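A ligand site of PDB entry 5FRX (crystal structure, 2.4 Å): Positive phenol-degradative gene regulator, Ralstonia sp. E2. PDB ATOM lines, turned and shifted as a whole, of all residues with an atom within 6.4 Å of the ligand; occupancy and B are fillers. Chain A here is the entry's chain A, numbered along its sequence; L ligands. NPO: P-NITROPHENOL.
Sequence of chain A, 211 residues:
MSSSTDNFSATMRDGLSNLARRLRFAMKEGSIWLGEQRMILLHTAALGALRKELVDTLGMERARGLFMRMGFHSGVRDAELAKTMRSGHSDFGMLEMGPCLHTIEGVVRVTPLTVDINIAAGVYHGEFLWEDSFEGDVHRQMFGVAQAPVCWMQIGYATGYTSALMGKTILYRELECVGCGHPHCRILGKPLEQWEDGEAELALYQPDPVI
CD2 of Leu 95 touches O3 of the ligand (3.5 Å). Gly 98 touches the ligand. Pro 99 touches the ligand. CG2 of Val 110 touches OH of the ligand, 3.3 Å away. Phe 128 touches the ligand. Tyr 157 touches the ligand (CE1 to C5, 3.8 Å). Tyr 161 touches the ligand. CD1 of Ile 187 touches C3 of the ligand, 3.7 Å away. Hydrophobic or aromatic side chains within 4 Å of the ligand: Leu 95, Pro 99, His 102, Val 110, Phe 128, Trp 130, Tyr 157, Tyr 161, Tyr 172 and Ile 187. 13 residues have an atom within 4 Å of the ligand: Leu 95, Gly 98, Pro 99, His 102, Val 110, Tyr 124, Phe 128, Trp 130, Tyr 157, Tyr 161, Thr 162, Tyr 172 and Ile 187. The nearest printed residue that does not touch the ligand is Ala 158 (4.03 Å).
O of Gly 98 is in hydrogen-bond range of OH of Tyr 157 (3.5 Å). The backbone carbonyl oxygen (O) of Ile 187 is in hydrogen-bond range of the backbone NH (N) of Phe 128 (3.0 Å). N of Gly 98 sits at hydrogen-bond distance from OH of Tyr 161 (3.1 Å). The backbone carbonyl oxygen of Ala 158 sits at hydrogen-bond distance from the side-chain hydroxyl of Thr 162 (3.3 Å). N of Tyr 172 lies within hydrogen-bond range of OG1 of Thr 159 (3.4 Å). OG1 of Thr 162 is in hydrogen-bond range of OH of Tyr 172 (2.8 Å). OH of Tyr 172 sits at hydrogen-bond distance from OH of Tyr 124, 2.8 Å away.
OH of the ligand lies within hydrogen-bond range of NE1 of Trp 130 (2.7 Å). O3 of the ligand lies within hydrogen-bond range of OH of Tyr 172 (2.6 Å). ND1 of His 102 sits at hydrogen-bond distance from OH of the ligand (2.6 Å). OG1 of Thr 162 sits at hydrogen-bond distance from O2 of the ligand (2.7 Å). The side-chain hydroxyl (OH) of Tyr 124 lies within hydrogen-bond range of an oxygen (O3) of the ligand, at 3.2 Å.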
ATOM      1  N   LEU A  95      20.581   8.648  19.021  1.00  0.00           N
ATOM      2  CA  LEU A  95      20.169   7.936  20.216  1.00  0.00           C
ATOM      3  C   LEU A  95      21.249   7.043  20.765  1.00  0.00           C
ATOM      4  O   LEU A  95      21.482   6.986  21.982  1.00  0.00           O
ATOM      5  CB  LEU A  95      18.919   7.115  19.910  1.00  0.00           C
ATOM      6  CG  LEU A  95      18.178   6.366  21.018  1.00  0.00           C
ATOM      7  CD1 LEU A  95      18.823   5.019  21.282  1.00  0.00           C
ATOM      8  CD2 LEU A  95      18.135   7.212  22.272  1.00  0.00           C
ATOM      9  N   MET A  97      24.385   7.016  20.793  1.00  0.00           N
ATOM     10  CA  MET A  97      25.519   7.609  21.497  1.00  0.00           C
ATOM     11  C   MET A  97      25.310   7.509  23.027  1.00  0.00           C
ATOM     12  O   MET A  97      26.255   7.279  23.767  1.00  0.00           O
ATOM     13  CB  MET A  97      25.732   9.055  21.050  1.00  0.00           C
ATOM     14  CG  MET A  97      26.459   9.143  19.698  1.00  0.00           C
ATOM     15  SD  MET A  97      26.757  10.804  19.022  1.00  0.00           S
ATOM     16  CE  MET A  97      25.258  11.073  18.082  1.00  0.00           C
ATOM     17  N   GLY A  98      24.073   7.676  23.473  1.00  0.00           N
ATOM     18  CA  GLY A  98      23.741   7.488  24.884  1.00  0.00           C
ATOM     19  C   GLY A  98      24.227   6.163  25.454  1.00  0.00           C
ATOM     20  O   GLY A  98      25.030   6.150  26.380  1.00  0.00           O
ATOM     21  N   PRO A  99      23.721   5.041  24.915  1.00  0.00           N
ATOM     22  CA  PRO A  99      24.193   3.714  25.301  1.00  0.00           C
ATOM     23  C   PRO A  99      25.714   3.587  25.201  1.00  0.00           C
ATOM     24  O   PRO A  99      26.352   3.024  26.104  1.00  0.00           O
ATOM     25  CB  PRO A  99      23.492   2.794  24.306  1.00  0.00           C
ATOM     26  CG  PRO A  99      22.208   3.453  24.085  1.00  0.00           C
ATOM     27  CD  PRO A  99      22.513   4.950  24.077  1.00  0.00           C
ATOM     28  N   CYS A 100      26.266   4.112  24.113  1.00  0.00           N
ATOM     29  CA  CYS A 100      27.694   4.161  23.906  1.00  0.00           C
ATOM     30  C   CYS A 100      28.420   4.866  25.044  1.00  0.00           C
ATOM     31  O   CYS A 100      29.339   4.303  25.632  1.00  0.00           O
ATOM     32  CB  CYS A 100      27.997   4.864  22.578  1.00  0.00           C
ATOM     33  SG  CYS A 100      27.660   3.816  21.134  1.00  0.00           S
ATOM     34  N   HIS A 102      27.376   5.602  28.018  1.00  0.00           N
ATOM     35  CA  HIS A 102      27.158   4.881  29.231  1.00  0.00           C
ATOM     36  C   HIS A 102      28.135   3.720  29.356  1.00  0.00           C
ATOM     37  O   HIS A 102      28.553   3.398  30.417  1.00  0.00           O
ATOM     38  CB  HIS A 102      25.725   4.369  29.316  1.00  0.00           C
ATOM     39  CG  HIS A 102      25.124   4.435  30.683  1.00  0.00           C
ATOM     40  ND1 HIS A 102      23.977   3.780  31.014  1.00  0.00           N
ATOM     41  CD2 HIS A 102      25.525   5.071  31.799  1.00  0.00           C
ATOM     42  CE1 HIS A 102      23.680   4.015  32.268  1.00  0.00           C
ATOM     43  NE2 HIS A 102      24.603   4.792  32.769  1.00  0.00           N
ATOM     44  N   VAL A 108      27.675   0.373  32.691  1.00  0.00           N
ATOM     45  CA  VAL A 108      26.953  -0.822  32.291  1.00  0.00           C
ATOM     46  C   VAL A 108      27.294  -1.139  30.842  1.00  0.00           C
ATOM     47  O   VAL A 108      27.728  -0.261  30.095  1.00  0.00           O
ATOM     48  CB  VAL A 108      25.418  -0.664  32.455  1.00  0.00           C
ATOM     49  CG1 VAL A 108      24.929   0.644  31.799  1.00  0.00           C
ATOM     50  CG2 VAL A 108      24.696  -1.858  31.853  1.00  0.00           C
ATOM     51  N   VAL A 110      25.560  -1.741  27.698  1.00  0.00           N
ATOM     52  CA  VAL A 110      24.235  -1.431  27.190  1.00  0.00           C
ATOM     53  C   VAL A 110      24.020  -2.181  25.902  1.00  0.00           C
ATOM     54  O   VAL A 110      24.910  -2.211  25.051  1.00  0.00           O
ATOM     55  CB  VAL A 110      24.060   0.089  26.960  1.00  0.00           C
ATOM     56  CG1 VAL A 110      22.627   0.394  26.619  1.00  0.00           C
ATOM     57  CG2 VAL A 110      24.486   0.848  28.191  1.00  0.00           C
ATOM     58  N   VAL A 115      14.606   0.004  19.114  1.00  0.00           N
ATOM     59  CA  VAL A 115      14.390   1.427  19.282  1.00  0.00           C
ATOM     60  C   VAL A 115      13.596   1.987  18.124  1.00  0.00           C
ATOM     61  O   VAL A 115      13.941   1.823  16.951  1.00  0.00           O
ATOM     62  CB  VAL A 115      15.713   2.206  19.418  1.00  0.00           C
ATOM     63  CG1 VAL A 115      15.455   3.717  19.490  1.00  0.00           C
ATOM     64  CG2 VAL A 115      16.475   1.753  20.647  1.00  0.00           C
ATOM     65  N   TYR A 124       9.137   8.263  20.550  1.00  0.00           N
ATOM     66  CA  TYR A 124      10.238   7.435  21.036  1.00  0.00           C
ATOM     67  C   TYR A 124       9.690   6.253  21.809  1.00  0.00           C
ATOM     68  O   TYR A 124       8.900   6.415  22.737  1.00  0.00           O
ATOM     69  CB  TYR A 124      11.200   8.228  21.951  1.00  0.00           C
ATOM     70  CG  TYR A 124      12.315   7.360  22.498  1.00  0.00           C
ATOM     71  CD1 TYR A 124      13.476   7.146  21.752  1.00  0.00           C
ATOM     72  CD2 TYR A 124      12.191   6.718  23.730  1.00  0.00           C
ATOM     73  CE1 TYR A 124      14.488   6.335  22.218  1.00  0.00           C
ATOM     74  CE2 TYR A 124      13.219   5.906  24.215  1.00  0.00           C
ATOM     75  CZ  TYR A 124      14.357   5.723  23.452  1.00  0.00           C
ATOM     76  OH  TYR A 124      15.376   4.921  23.896  1.00  0.00           O
ATOM     77  N   PHE A 128      16.094  -1.735  26.270  1.00  0.00           N
ATOM     78  CA  PHE A 128      17.508  -2.052  26.283  1.00  0.00           C
ATOM     79  C   PHE A 128      17.805  -3.165  27.266  1.00  0.00           C
ATOM     80  O   PHE A 128      17.094  -3.341  28.256  1.00  0.00           O
ATOM     81  CB  PHE A 128      18.323  -0.797  26.631  1.00  0.00           C
ATOM     82  CG  PHE A 128      18.096   0.348  25.691  1.00  0.00           C
ATOM     83  CD1 PHE A 128      16.966   1.121  25.776  1.00  0.00           C
ATOM     84  CD2 PHE A 128      19.030   0.643  24.723  1.00  0.00           C
ATOM     85  CE1 PHE A 128      16.769   2.165  24.908  1.00  0.00           C
ATOM     86  CE2 PHE A 128      18.843   1.692  23.847  1.00  0.00           C
ATOM     87  CZ  PHE A 128      17.711   2.454  23.944  1.00  0.00           C
ATOM     88  N   LEU A 129      18.859  -3.917  26.966  1.00  0.00           N
ATOM     89  CA  LEU A 129      19.443  -4.854  27.916  1.00  0.00           C
ATOM     90  C   LEU A 129      20.639  -4.170  28.613  1.00  0.00           C
ATOM     91  O   LEU A 129      21.362  -3.392  27.981  1.00  0.00           O
ATOM     92  CB  LEU A 129      19.894  -6.126  27.176  1.00  0.00           C
ATOM     93  CG  LEU A 129      20.762  -7.149  27.923  1.00  0.00           C
ATOM     94  CD1 LEU A 129      19.895  -8.049  28.792  1.00  0.00           C
ATOM     95  CD2 LEU A 129      21.641  -7.962  26.961  1.00  0.00           C
ATOM     96  N   TRP A 130      20.815  -4.453  29.907  1.00  0.00           N
ATOM     97  CA  TRP A 130      21.969  -3.955  30.688  1.00  0.00           C
ATOM     98  C   TRP A 130      22.797  -5.098  31.258  1.00  0.00           C
ATOM     99  O   TRP A 130      22.373  -5.770  32.181  1.00  0.00           O
ATOM    100  CB  TRP A 130      21.503  -3.077  31.865  1.00  0.00           C
ATOM    101  CG  TRP A 130      21.259  -1.625  31.545  1.00  0.00           C
ATOM    102  CD1 TRP A 130      21.677  -0.936  30.448  1.00  0.00           C
ATOM    103  CD2 TRP A 130      20.511  -0.685  32.342  1.00  0.00           C
ATOM    104  NE1 TRP A 130      21.236   0.374  30.514  1.00  0.00           N
ATOM    105  CE2 TRP A 130      20.512   0.547  31.668  1.00  0.00           C
ATOM    106  CE3 TRP A 130      19.832  -0.776  33.569  1.00  0.00           C
ATOM    107  CZ2 TRP A 130      19.880   1.683  32.164  1.00  0.00           C
ATOM    108  CZ3 TRP A 130      19.187   0.358  34.061  1.00  0.00           C
ATOM    109  CH2 TRP A 130      19.224   1.564  33.364  1.00  0.00           C
ATOM    110  N   GLN A 154      21.678   4.765  37.049  1.00  0.00           N
ATOM    111  CA  GLN A 154      21.720   4.317  35.662  1.00  0.00           C
ATOM    112  C   GLN A 154      20.420   4.625  34.930  1.00  0.00           C
ATOM    113  O   GLN A 154      20.435   4.932  33.746  1.00  0.00           O
ATOM    114  CB  GLN A 154      22.003   2.825  35.596  1.00  0.00           C
ATOM    115  CG  GLN A 154      23.309   2.443  36.270  1.00  0.00           C
ATOM    116  CD  GLN A 154      23.570   0.952  36.217  1.00  0.00           C
ATOM    117  OE1 GLN A 154      24.519   0.466  36.831  1.00  0.00           O
ATOM    118  NE2 GLN A 154      22.741   0.222  35.487  1.00  0.00           N
ATOM    119  N   TYR A 157      20.106   8.356  34.192  1.00  0.00           N
ATOM    120  CA  TYR A 157      20.913   8.721  33.040  1.00  0.00           C
ATOM    121  C   TYR A 157      20.132   8.492  31.749  1.00  0.00           C
ATOM    122  O   TYR A 157      20.072   9.382  30.900  1.00  0.00           O
ATOM    123  CB  TYR A 157      22.220   7.923  33.026  1.00  0.00           C
ATOM    124  CG  TYR A 157      23.132   8.199  31.841  1.00  0.00           C
ATOM    125  CD1 TYR A 157      22.822   7.680  30.589  1.00  0.00           C
ATOM    126  CD2 TYR A 157      24.307   8.938  31.980  1.00  0.00           C
ATOM    127  CE1 TYR A 157      23.601   7.910  29.515  1.00  0.00           C
ATOM    128  CE2 TYR A 157      25.134   9.172  30.880  1.00  0.00           C
ATOM    129  CZ  TYR A 157      24.767   8.644  29.640  1.00  0.00           C
ATOM    130  OH  TYR A 157      25.539   8.835  28.505  1.00  0.00           O
ATOM    131  N   ALA A 158      19.532   7.313  31.608  1.00  0.00           N
ATOM    132  CA  ALA A 158      18.697   7.015  30.456  1.00  0.00           C
ATOM    133  C   ALA A 158      17.644   8.113  30.259  1.00  0.00           C
ATOM    134  O   ALA A 158      17.534   8.706  29.183  1.00  0.00           O
ATOM    135  CB  ALA A 158      18.029   5.666  30.619  1.00  0.00           C
ATOM    136  N   THR A 159      16.885   8.368  31.322  1.00  0.00           N
ATOM    137  CA  THR A 159      15.895   9.426  31.383  1.00  0.00           C
ATOM    138  C   THR A 159      16.448  10.788  31.013  1.00  0.00           C
ATOM    139  O   THR A 159      15.818  11.532  30.280  1.00  0.00           O
ATOM    140  CB  THR A 159      15.310   9.527  32.793  1.00  0.00           C
ATOM    141  OG1 THR A 159      14.736   8.256  33.154  1.00  0.00           O
ATOM    142  CG2 THR A 159      14.256  10.618  32.886  1.00  0.00           C
ATOM    143  N   TYR A 161      19.497  11.589  29.381  1.00  0.00           N
ATOM    144  CA  TYR A 161      19.971  11.593  28.010  1.00  0.00           C
ATOM    145  C   TYR A 161      18.858  11.745  26.962  1.00  0.00           C
ATOM    146  O   TYR A 161      18.958  12.558  26.033  1.00  0.00           O
ATOM    147  CB  TYR A 161      20.748  10.312  27.690  1.00  0.00           C
ATOM    148  CG  TYR A 161      21.423  10.353  26.317  1.00  0.00           C
ATOM    149  CD1 TYR A 161      20.704  10.032  25.153  1.00  0.00           C
ATOM    150  CD2 TYR A 161      22.772  10.745  26.170  1.00  0.00           C
ATOM    151  CE1 TYR A 161      21.300  10.087  23.899  1.00  0.00           C
ATOM    152  CE2 TYR A 161      23.376  10.794  24.898  1.00  0.00           C
ATOM    153  CZ  TYR A 161      22.616  10.464  23.765  1.00  0.00           C
ATOM    154  OH  TYR A 161      23.168  10.503  22.496  1.00  0.00           O
ATOM    155  N   THR A 162      17.794  10.965  27.115  1.00  0.00           N
ATOM    156  CA  THR A 162      16.821  10.803  26.038  1.00  0.00           C
ATOM    157  C   THR A 162      15.859  11.945  26.024  1.00  0.00           C
ATOM    158  O   THR A 162      15.406  12.355  24.971  1.00  0.00           O
ATOM    159  CB  THR A 162      16.045   9.475  26.149  1.00  0.00           C
ATOM    160  OG1 THR A 162      16.973   8.410  25.951  1.00  0.00           O
ATOM    161  CG2 THR A 162      14.955   9.372  25.108  1.00  0.00           C
ATOM    162  N   TYR A 172      12.270   6.277  31.993  1.00  0.00           N
ATOM    163  CA  TYR A 172      12.545   4.841  31.920  1.00  0.00           C
ATOM    164  C   TYR A 172      12.219   4.131  33.229  1.00  0.00           C
ATOM    165  O   TYR A 172      12.284   4.721  34.304  1.00  0.00           O
ATOM    166  CB  TYR A 172      14.015   4.567  31.601  1.00  0.00           C
ATOM    167  CG  TYR A 172      14.514   4.927  30.230  1.00  0.00           C
ATOM    168  CD1 TYR A 172      14.622   6.260  29.832  1.00  0.00           C
ATOM    169  CD2 TYR A 172      14.923   3.945  29.354  1.00  0.00           C
ATOM    170  CE1 TYR A 172      15.110   6.581  28.589  1.00  0.00           C
ATOM    171  CE2 TYR A 172      15.412   4.267  28.111  1.00  0.00           C
ATOM    172  CZ  TYR A 172      15.507   5.583  27.735  1.00  0.00           C
ATOM    173  OH  TYR A 172      16.003   5.885  26.500  1.00  0.00           O
ATOM    174  N   ILE A 187      15.300  -2.540  30.604  1.00  0.00           N
ATOM    175  CA  ILE A 187      14.634  -1.257  30.770  1.00  0.00           C
ATOM    176  C   ILE A 187      13.804  -0.880  29.553  1.00  0.00           C
ATOM    177  O   ILE A 187      14.086  -1.287  28.425  1.00  0.00           O
ATOM    178  CB  ILE A 187      15.661  -0.106  31.056  1.00  0.00           C
ATOM    179  CG1 ILE A 187      16.240   0.428  29.731  1.00  0.00           C
ATOM    180  CG2 ILE A 187      16.758  -0.579  32.042  1.00  0.00           C
ATOM    181  CD1 ILE A 187      17.491   1.321  29.898  1.00  0.00           C
HETATM  182  C1  NPO L   1      19.942   5.113  26.844  1.00  0.00           C
HETATM  183  C2  NPO L   1      19.488   3.854  27.186  1.00  0.00           C
HETATM  184  C3  NPO L   1      20.217   3.076  28.058  1.00  0.00           C
HETATM  185  C4  NPO L   1      21.400   3.557  28.588  1.00  0.00           C
HETATM  186  C5  NPO L   1      21.867   4.818  28.251  1.00  0.00           C
HETATM  187  C6  NPO L   1      21.127   5.604  27.383  1.00  0.00           C
HETATM  188  OH  NPO L   1      22.131   2.752  29.468  1.00  0.00           O
HETATM  189  N1  NPO L   1      19.162   5.905  25.957  1.00  0.00           N
HETATM  190  O2  NPO L   1      19.388   7.251  25.909  1.00  0.00           O
HETATM  191  O3  NPO L   1      18.253   5.405  25.281  1.00  0.00           O
